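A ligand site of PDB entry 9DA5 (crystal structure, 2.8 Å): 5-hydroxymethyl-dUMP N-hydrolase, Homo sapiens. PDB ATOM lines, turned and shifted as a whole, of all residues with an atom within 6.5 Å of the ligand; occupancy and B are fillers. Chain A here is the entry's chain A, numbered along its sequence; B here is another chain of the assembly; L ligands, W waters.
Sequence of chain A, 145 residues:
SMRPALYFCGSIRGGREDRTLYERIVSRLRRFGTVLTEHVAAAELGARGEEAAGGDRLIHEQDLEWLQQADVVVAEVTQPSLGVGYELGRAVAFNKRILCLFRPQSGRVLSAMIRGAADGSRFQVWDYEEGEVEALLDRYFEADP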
ATOM      1  N   TYR A   7      -1.666  -8.757   9.823  1.00  0.00           N
ATOM      2  CA  TYR A   7      -0.546  -8.466  10.695  1.00  0.00           C
ATOM      3  C   TYR A   7      -0.752  -9.237  12.000  1.00  0.00           C
ATOM      4  O   TYR A   7      -1.820  -9.141  12.608  1.00  0.00           O
ATOM      5  CB  TYR A   7      -0.455  -6.960  10.938  1.00  0.00           C
ATOM      6  CG  TYR A   7       0.829  -6.475  11.607  1.00  0.00           C
ATOM      7  CD1 TYR A   7       1.019  -6.617  12.985  1.00  0.00           C
ATOM      8  CD2 TYR A   7       1.826  -5.830  10.859  1.00  0.00           C
ATOM      9  CE1 TYR A   7       2.143  -6.172  13.590  1.00  0.00           C
ATOM     10  CE2 TYR A   7       2.972  -5.378  11.456  1.00  0.00           C
ATOM     11  CZ  TYR A   7       3.131  -5.549  12.836  1.00  0.00           C
ATOM     12  OH  TYR A   7       4.268  -5.105  13.476  1.00  0.00           O
ATOM     13  N   PHE A   8       0.259  -9.991  12.418  1.00  0.00           N
ATOM     14  CA  PHE A   8       0.162 -10.769  13.641  1.00  0.00           C
ATOM     15  C   PHE A   8       1.082 -10.188  14.710  1.00  0.00           C
ATOM     16  O   PHE A   8       2.293 -10.110  14.495  1.00  0.00           O
ATOM     17  CB  PHE A   8       0.550 -12.226  13.423  1.00  0.00           C
ATOM     18  CG  PHE A   8       0.514 -13.015  14.694  1.00  0.00           C
ATOM     19  CD1 PHE A   8      -0.686 -13.425  15.237  1.00  0.00           C
ATOM     20  CD2 PHE A   8       1.675 -13.288  15.390  1.00  0.00           C
ATOM     21  CE1 PHE A   8      -0.719 -14.130  16.413  1.00  0.00           C
ATOM     22  CE2 PHE A   8       1.630 -13.990  16.588  1.00  0.00           C
ATOM     23  CZ  PHE A   8       0.443 -14.416  17.088  1.00  0.00           C
ATOM     24  N   CYS A   9       0.510  -9.849  15.881  1.00  0.00           N
ATOM     25  CA  CYS A   9       1.244  -9.415  17.060  1.00  0.00           C
ATOM     26  C   CYS A   9       1.234 -10.493  18.140  1.00  0.00           C
ATOM     27  O   CYS A   9       0.189 -11.087  18.428  1.00  0.00           O
ATOM     28  CB  CYS A   9       0.654  -8.148  17.701  1.00  0.00           C
ATOM     29  SG  CYS A   9      -0.150  -6.994  16.654  1.00  0.00           S
ATOM     30  N   GLY A  10       2.385 -10.666  18.784  1.00  0.00           N
ATOM     31  CA  GLY A  10       2.513 -11.590  19.890  1.00  0.00           C
ATOM     32  C   GLY A  10       3.872 -11.418  20.495  1.00  0.00           C
ATOM     33  O   GLY A  10       4.847 -11.162  19.774  1.00  0.00           O
ATOM     34  N   SER A  11       3.952 -11.580  21.814  1.00  0.00           N
ATOM     35  CA  SER A  11       5.136 -11.230  22.590  1.00  0.00           C
ATOM     36  C   SER A  11       6.405 -11.850  22.019  1.00  0.00           C
ATOM     37  O   SER A  11       6.395 -12.965  21.493  1.00  0.00           O
ATOM     38  CB  SER A  11       4.903 -11.670  24.041  1.00  0.00           C
ATOM     39  OG  SER A  11       6.092 -11.616  24.812  1.00  0.00           O
ATOM     40  N   ILE A  12       7.513 -11.103  22.099  1.00  0.00           N
ATOM     41  CA  ILE A  12       8.841 -11.654  21.785  1.00  0.00           C
ATOM     42  C   ILE A  12       9.829 -11.310  22.887  1.00  0.00           C
ATOM     43  O   ILE A  12      10.293 -12.206  23.598  1.00  0.00           O
ATOM     44  CB  ILE A  12       9.382 -11.173  20.428  1.00  0.00           C
ATOM     45  CG1 ILE A  12       8.646 -11.843  19.278  1.00  0.00           C
ATOM     46  CG2 ILE A  12      10.882 -11.469  20.335  1.00  0.00           C
ATOM     47  CD1 ILE A  12       9.198 -11.446  17.944  1.00  0.00           C
ATOM     48  N   ARG A  13      10.185 -10.022  23.034  1.00  0.00           N
ATOM     49  CA  ARG A  13      11.085  -9.637  24.117  1.00  0.00           C
ATOM     50  C   ARG A  13      10.384  -9.583  25.470  1.00  0.00           C
ATOM     51  O   ARG A  13      11.073  -9.545  26.507  1.00  0.00           O
ATOM     52  CB  ARG A  13      11.748  -8.292  23.827  1.00  0.00           C
ATOM     53  CG  ARG A  13      12.665  -8.225  22.624  1.00  0.00           C
ATOM     54  CD  ARG A  13      13.930  -7.416  22.874  1.00  0.00           C
ATOM     55  NE  ARG A  13      14.750  -7.276  21.666  1.00  0.00           N
ATOM     56  CZ  ARG A  13      15.120  -6.122  21.130  1.00  0.00           C
ATOM     57  NH1 ARG A  13      14.720  -4.965  21.626  1.00  0.00           N
ATOM     58  NH2 ARG A  13      15.938  -6.135  20.082  1.00  0.00           N
ATOM     59  N   GLY A  14       9.048  -9.559  25.517  1.00  0.00           N
ATOM     60  CA  GLY A  14       8.403  -9.589  26.815  1.00  0.00           C
ATOM     61  C   GLY A  14       8.329 -10.973  27.418  1.00  0.00           C
ATOM     62  O   GLY A  14       7.804 -11.166  28.532  1.00  0.00           O
ATOM     63  N   GLY A  15       8.845 -11.952  26.650  1.00  0.00           N
ATOM     64  CA  GLY A  15       8.783 -13.380  26.950  1.00  0.00           C
ATOM     65  C   GLY A  15       8.296 -14.144  25.730  1.00  0.00           C
ATOM     66  O   GLY A  15       7.408 -13.644  25.031  1.00  0.00           O
ATOM     67  N   THR A  37       3.939  -9.993   8.721  1.00  0.00           N
ATOM     68  CA  THR A  37       4.885 -10.153   9.818  1.00  0.00           C
ATOM     69  C   THR A  37       5.717 -11.428   9.685  1.00  0.00           C
ATOM     70  O   THR A  37       5.307 -12.410   9.057  1.00  0.00           O
ATOM     71  CB  THR A  37       4.108 -10.103  11.147  1.00  0.00           C
ATOM     72  OG1 THR A  37       3.274 -11.264  11.288  1.00  0.00           O
ATOM     73  CG2 THR A  37       3.244  -8.885  11.169  1.00  0.00           C
ATOM     74  N   GLU A  38       6.921 -11.373  10.250  1.00  0.00           N
ATOM     75  CA  GLU A  38       7.887 -12.469  10.263  1.00  0.00           C
ATOM     76  C   GLU A  38       8.152 -13.065   8.877  1.00  0.00           C
ATOM     77  O   GLU A  38       7.749 -12.494   7.855  1.00  0.00           O
ATOM     78  CB  GLU A  38       7.427 -13.571  11.218  1.00  0.00           C
ATOM     79  CG  GLU A  38       6.973 -13.055  12.592  1.00  0.00           C
ATOM     80  CD  GLU A  38       5.606 -13.634  13.054  1.00  0.00           C
ATOM     81  OE1 GLU A  38       4.595 -13.481  12.327  1.00  0.00           O
ATOM     82  OE2 GLU A  38       5.542 -14.216  14.163  1.00  0.00           O
ATOM     83  N   ASP A  56      17.140  -1.883  15.942  1.00  0.00           N
ATOM     84  CA  ASP A  56      15.763  -1.787  16.412  1.00  0.00           C
ATOM     85  C   ASP A  56      15.001  -0.732  15.629  1.00  0.00           C
ATOM     86  O   ASP A  56      13.779  -0.846  15.449  1.00  0.00           O
ATOM     87  CB  ASP A  56      15.756  -1.471  17.904  1.00  0.00           C
ATOM     88  CG  ASP A  56      16.165  -2.651  18.753  1.00  0.00           C
ATOM     89  OD1 ASP A  56      16.675  -3.650  18.184  1.00  0.00           O
ATOM     90  OD2 ASP A  56      15.969  -2.618  19.969  1.00  0.00           O
ATOM     91  N   ILE A  59      13.632  -2.560  12.483  1.00  0.00           N
ATOM     92  CA  ILE A  59      12.456  -3.303  12.929  1.00  0.00           C
ATOM     93  C   ILE A  59      11.281  -2.363  13.126  1.00  0.00           C
ATOM     94  O   ILE A  59      10.218  -2.532  12.503  1.00  0.00           O
ATOM     95  CB  ILE A  59      12.804  -4.077  14.207  1.00  0.00           C
ATOM     96  CG1 ILE A  59      14.015  -4.957  13.935  1.00  0.00           C
ATOM     97  CG2 ILE A  59      11.578  -4.867  14.698  1.00  0.00           C
ATOM     98  CD1 ILE A  59      14.480  -5.730  15.089  1.00  0.00           C
ATOM     99  N   ASP A  63       7.993  -2.824  10.516  1.00  0.00           N
ATOM    100  CA  ASP A  63       6.663  -3.245  10.979  1.00  0.00           C
ATOM    101  C   ASP A  63       5.642  -2.120  10.975  1.00  0.00           C
ATOM    102  O   ASP A  63       4.441  -2.378  10.827  1.00  0.00           O
ATOM    103  CB  ASP A  63       6.748  -3.896  12.362  1.00  0.00           C
ATOM    104  CG  ASP A  63       7.755  -5.021  12.438  1.00  0.00           C
ATOM    105  OD1 ASP A  63       8.956  -4.762  12.289  1.00  0.00           O
ATOM    106  OD2 ASP A  63       7.298  -6.172  12.580  1.00  0.00           O
ATOM    107  N   PRO A  80       2.303 -10.418  28.668  1.00  0.00           N
ATOM    108  CA  PRO A  80       2.418  -8.956  28.642  1.00  0.00           C
ATOM    109  C   PRO A  80       3.676  -8.560  27.885  1.00  0.00           C
ATOM    110  O   PRO A  80       4.723  -9.184  28.044  1.00  0.00           O
ATOM    111  CB  PRO A  80       2.484  -8.585  30.122  1.00  0.00           C
ATOM    112  CG  PRO A  80       1.777  -9.670  30.788  1.00  0.00           C
ATOM    113  CD  PRO A  80       2.201 -10.900  30.045  1.00  0.00           C
ATOM    114  N   SER A  81       3.539  -7.537  27.038  1.00  0.00           N
ATOM    115  CA  SER A  81       4.588  -7.115  26.118  1.00  0.00           C
ATOM    116  C   SER A  81       4.384  -5.636  25.741  1.00  0.00           C
ATOM    117  O   SER A  81       3.289  -5.234  25.371  1.00  0.00           O
ATOM    118  CB  SER A  81       4.589  -8.000  24.863  1.00  0.00           C
ATOM    119  OG  SER A  81       5.193  -7.365  23.726  1.00  0.00           O
ATOM    120  N   LEU A  82       5.448  -4.849  25.843  1.00  0.00           N
ATOM    121  CA  LEU A  82       5.352  -3.473  25.338  1.00  0.00           C
ATOM    122  C   LEU A  82       5.112  -3.474  23.839  1.00  0.00           C
ATOM    123  O   LEU A  82       4.206  -2.785  23.341  1.00  0.00           O
ATOM    124  CB  LEU A  82       6.609  -2.670  25.688  1.00  0.00           C
ATOM    125  CG  LEU A  82       7.023  -2.412  27.152  1.00  0.00           C
ATOM    126  CD1 LEU A  82       8.434  -1.780  27.267  1.00  0.00           C
ATOM    127  CD2 LEU A  82       5.981  -1.567  27.907  1.00  0.00           C
ATOM    128  N   GLY A  83       5.900  -4.254  23.091  1.00  0.00           N
ATOM    129  CA  GLY A  83       5.793  -4.227  21.643  1.00  0.00           C
ATOM    130  C   GLY A  83       4.385  -4.444  21.126  1.00  0.00           C
ATOM    131  O   GLY A  83       3.891  -3.659  20.313  1.00  0.00           O
ATOM    132  N   VAL A  84       3.720  -5.504  21.606  1.00  0.00           N
ATOM    133  CA  VAL A  84       2.323  -5.795  21.253  1.00  0.00           C
ATOM    134  C   VAL A  84       1.425  -4.623  21.604  1.00  0.00           C
ATOM    135  O   VAL A  84       0.598  -4.175  20.805  1.00  0.00           O
ATOM    136  CB  VAL A  84       1.869  -7.109  21.945  1.00  0.00           C
ATOM    137  CG1 VAL A  84       0.409  -7.431  21.666  1.00  0.00           C
ATOM    138  CG2 VAL A  84       2.785  -8.251  21.558  1.00  0.00           C
ATOM    139  N   GLU A  87       2.039  -1.799  19.077  1.00  0.00           N
ATOM    140  CA  GLU A  87       1.475  -2.103  17.768  1.00  0.00           C
ATOM    141  C   GLU A  87      -0.024  -1.846  17.756  1.00  0.00           C
ATOM    142  O   GLU A  87      -0.556  -1.246  16.816  1.00  0.00           O
ATOM    143  CB  GLU A  87       1.784  -3.550  17.368  1.00  0.00           C
ATOM    144  CG  GLU A  87       3.280  -3.809  17.161  1.00  0.00           C
ATOM    145  CD  GLU A  87       3.638  -5.265  16.788  1.00  0.00           C
ATOM    146  OE1 GLU A  87       2.926  -6.218  17.181  1.00  0.00           O
ATOM    147  OE2 GLU A  87       4.695  -5.426  16.132  1.00  0.00           O
ATOM    148  N   VAL B 109      16.036  -7.107  27.824  1.00  0.00           N
ATOM    149  CA  VAL B 109      16.271  -6.255  26.671  1.00  0.00           C
ATOM    150  C   VAL B 109      14.971  -5.525  26.370  1.00  0.00           C
ATOM    151  O   VAL B 109      13.924  -6.159  26.171  1.00  0.00           O
ATOM    152  CB  VAL B 109      16.722  -7.048  25.448  1.00  0.00           C
ATOM    153  CG1 VAL B 109      17.248  -6.075  24.388  1.00  0.00           C
ATOM    154  CG2 VAL B 109      17.769  -8.083  25.824  1.00  0.00           C
ATOM    155  N   LEU B 110      15.029  -4.199  26.342  1.00  0.00           N
ATOM    156  CA  LEU B 110      13.839  -3.421  26.050  1.00  0.00           C
ATOM    157  C   LEU B 110      13.350  -3.708  24.639  1.00  0.00           C
ATOM    158  O   LEU B 110      14.129  -3.991  23.735  1.00  0.00           O
ATOM    159  CB  LEU B 110      14.158  -1.947  26.207  1.00  0.00           C
ATOM    160  CG  LEU B 110      13.136  -0.971  25.676  1.00  0.00           C
ATOM    161  CD1 LEU B 110      11.900  -1.060  26.543  1.00  0.00           C
ATOM    162  CD2 LEU B 110      13.752   0.425  25.697  1.00  0.00           C
ATOM    163  N   SER B 111      12.023  -3.647  24.471  1.00  0.00           N
ATOM    164  CA  SER B 111      11.361  -3.864  23.191  1.00  0.00           C
ATOM    165  C   SER B 111      11.933  -2.985  22.090  1.00  0.00           C
ATOM    166  O   SER B 111      12.109  -1.782  22.268  1.00  0.00           O
ATOM    167  CB  SER B 111       9.890  -3.555  23.312  1.00  0.00           C
ATOM    168  OG  SER B 111       9.272  -3.868  22.097  1.00  0.00           O
ATOM    169  N   ALA B 112      12.146  -3.603  20.912  1.00  0.00           N
ATOM    170  CA  ALA B 112      12.585  -2.835  19.748  1.00  0.00           C
ATOM    171  C   ALA B 112      11.540  -1.839  19.295  1.00  0.00           C
ATOM    172  O   ALA B 112      11.908  -0.891  18.589  1.00  0.00           O
ATOM    173  CB  ALA B 112      12.937  -3.747  18.588  1.00  0.00           C
ATOM    174  N   MET B 113      10.263  -2.046  19.630  1.00  0.00           N
ATOM    175  CA  MET B 113       9.237  -1.061  19.318  1.00  0.00           C
ATOM    176  C   MET B 113       9.423   0.205  20.123  1.00  0.00           C
ATOM    177  O   MET B 113       8.883   1.234  19.729  1.00  0.00           O
ATOM    178  CB  MET B 113       7.817  -1.566  19.588  1.00  0.00           C
ATOM    179  CG  MET B 113       7.299  -2.620  18.640  1.00  0.00           C
ATOM    180  SD  MET B 113       8.047  -2.588  16.991  1.00  0.00           S
ATOM    181  CE  MET B 113       7.020  -1.301  16.232  1.00  0.00           C
HETATM  182  C1  LIG L   1       9.823  -8.135  15.742  1.00  0.00           C
HETATM  183  C2  LIG L   1      11.724  -8.307  17.075  1.00  0.00           C
HETATM  184  C3  LIG L   1       5.738  -8.575  17.988  1.00  0.00           C
HETATM  185  C4  LIG L   1       5.972  -7.539  18.911  1.00  0.00           C
HETATM  186  C5  LIG L   1       6.722  -8.101  20.197  1.00  0.00           C
HETATM  187  C6  LIG L   1       6.894  -6.526  18.275  1.00  0.00           C
HETATM  188  C7  LIG L   1       7.959  -6.525  16.291  1.00  0.00           C
HETATM  189  C8  LIG L   1       9.340  -7.125  16.579  1.00  0.00           C
HETATM  190  C9  LIG L   1      10.060  -6.743  17.674  1.00  0.00           C
HETATM  191  C10 LIG L   1      11.257  -7.324  17.933  1.00  0.00           C
HETATM  192  C11 LIG L   1      12.083  -6.912  19.158  1.00  0.00           C
HETATM  193  C12 LIG L   1       6.392  -8.193  16.672  1.00  0.00           C
HETATM  194  N1  LIG L   1       7.348  -7.166  17.082  1.00  0.00           N
HETATM  195  N2  LIG L   1      11.025  -8.710  15.993  1.00  0.00           N
HETATM  196  O1  LIG L   1       4.293  -8.678  17.801  1.00  0.00           O
HETATM  197  O2  LIG L   1       7.182  -7.018  20.934  1.00  0.00           O
HETATM  198  O3  LIG L   1       7.688  -8.467  23.033  1.00  0.00           O
HETATM  199  O4  LIG L   1       9.516  -7.811  21.803  1.00  0.00           O
HETATM  200  O5  LIG L   1       8.348  -6.251  23.135  1.00  0.00           O
HETATM  201  O6  LIG L   1      11.269  -6.649  20.269  1.00  0.00           O
HETATM  202  P1  LIG L   1       8.183  -7.373  22.205  1.00  0.00           P
HETATM  203  O   HOH W   1       8.009  -5.810  25.838  1.00  0.00           O
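O4 of the ligand lies within hydrogen-bond range of N of Arg 13 (2.6 Å).
OG of Ser 111 of chain B lies within hydrogen-bond range of O5 of the ligand (2.8 Å).
O3 of the ligand sits at hydrogen-bond distance from N of Ile 12 (2.8 Å).
OG of Ser 81 is in hydrogen-bond range of O3 of the ligand.
A nitrogen (N1) of the ligand lies within salt-bridge range of the side-chain carboxylate (OE2) of Glu 87 (3.3 Å).
N of Gly 10 lies within hydrogen-bond range of O1 of the ligand.
The backbone carbonyl oxygen of Gly 10 is in hydrogen-bond range of an oxygen (O1) of the ligand (3.2 Å).
An oxygen (O3) of the ligand is in hydrogen-bond range of the backbone NH of Gly 14 (3.0 Å).
N of Gly 83 lies within hydrogen-bond range of O5 of the ligand (3.2 Å).
O6 of the ligand sits at hydrogen-bond distance from N of Ala 112 of chain B (3.2 Å).
Merely in contact with the ligand: Cys 9 (3.2 Å), Ser 11 (3.8 Å), Ile 59 (3.7 Å), Asp 63 (3.8 Å), Val 84 (3.8 Å) and Met 113 of chain B (3.9 Å).
Hydrophobic or aromatic side chains within 4 Å of the ligand: Ile 12, Ile 59, Ala 112 of chain B and Met 113 of chain B.
Within 4 Å of the ligand: Cys 9, Gly 10, Ser 11, Ile 12, Arg 13, Gly 14, Ile 59, Asp 63, Ser 81, Gly 83, Val 84, Glu 87, Ser 111 of chain B, Ala 112 of chain B and Met 113 of chain B.
The nearest printed residue that does not touch the ligand is Phe 8 (4.1 Å).
The side-chain carboxylate (OD2) of Asp 56 is in salt-bridge range of the guanidinium group (NH1) of Arg 13 (3.1 Å).
The side-chain hydroxyl (OG) of Ser 81 sits at hydrogen-bond distance from the backbone NH (N) of Gly 83, at 3.3 Å.
The side-chain hydroxyl of Ser 81 sits at hydrogen-bond distance from the backbone NH of Val 84 (3.2 Å).
OE1 of Glu 87 lies close to SG of Cys 9, at 3.2 Å.
The side-chain carboxylate of Glu 87 is in hydrogen-bond range of the side-chain hydroxyl of Tyr 7, at 2.7 Å.
The backbone carbonyl oxygen of Ile 59 lies close to the side-chain carboxylate of Asp 63.
The side-chain hydroxyl of Ser 11 sits at hydrogen-bond distance from the backbone carbonyl oxygen of Gly 15 (2.4 Å).
The side-chain hydroxyl (OH) of Tyr 7 lies close to the side-chain carboxylate (OD2) of Asp 63, at 3.3 Å.
Water W1 bridges the backbone NH of Leu 82 (2.7 Å) and an oxygen (O5) of the ligand (2.8 Å).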
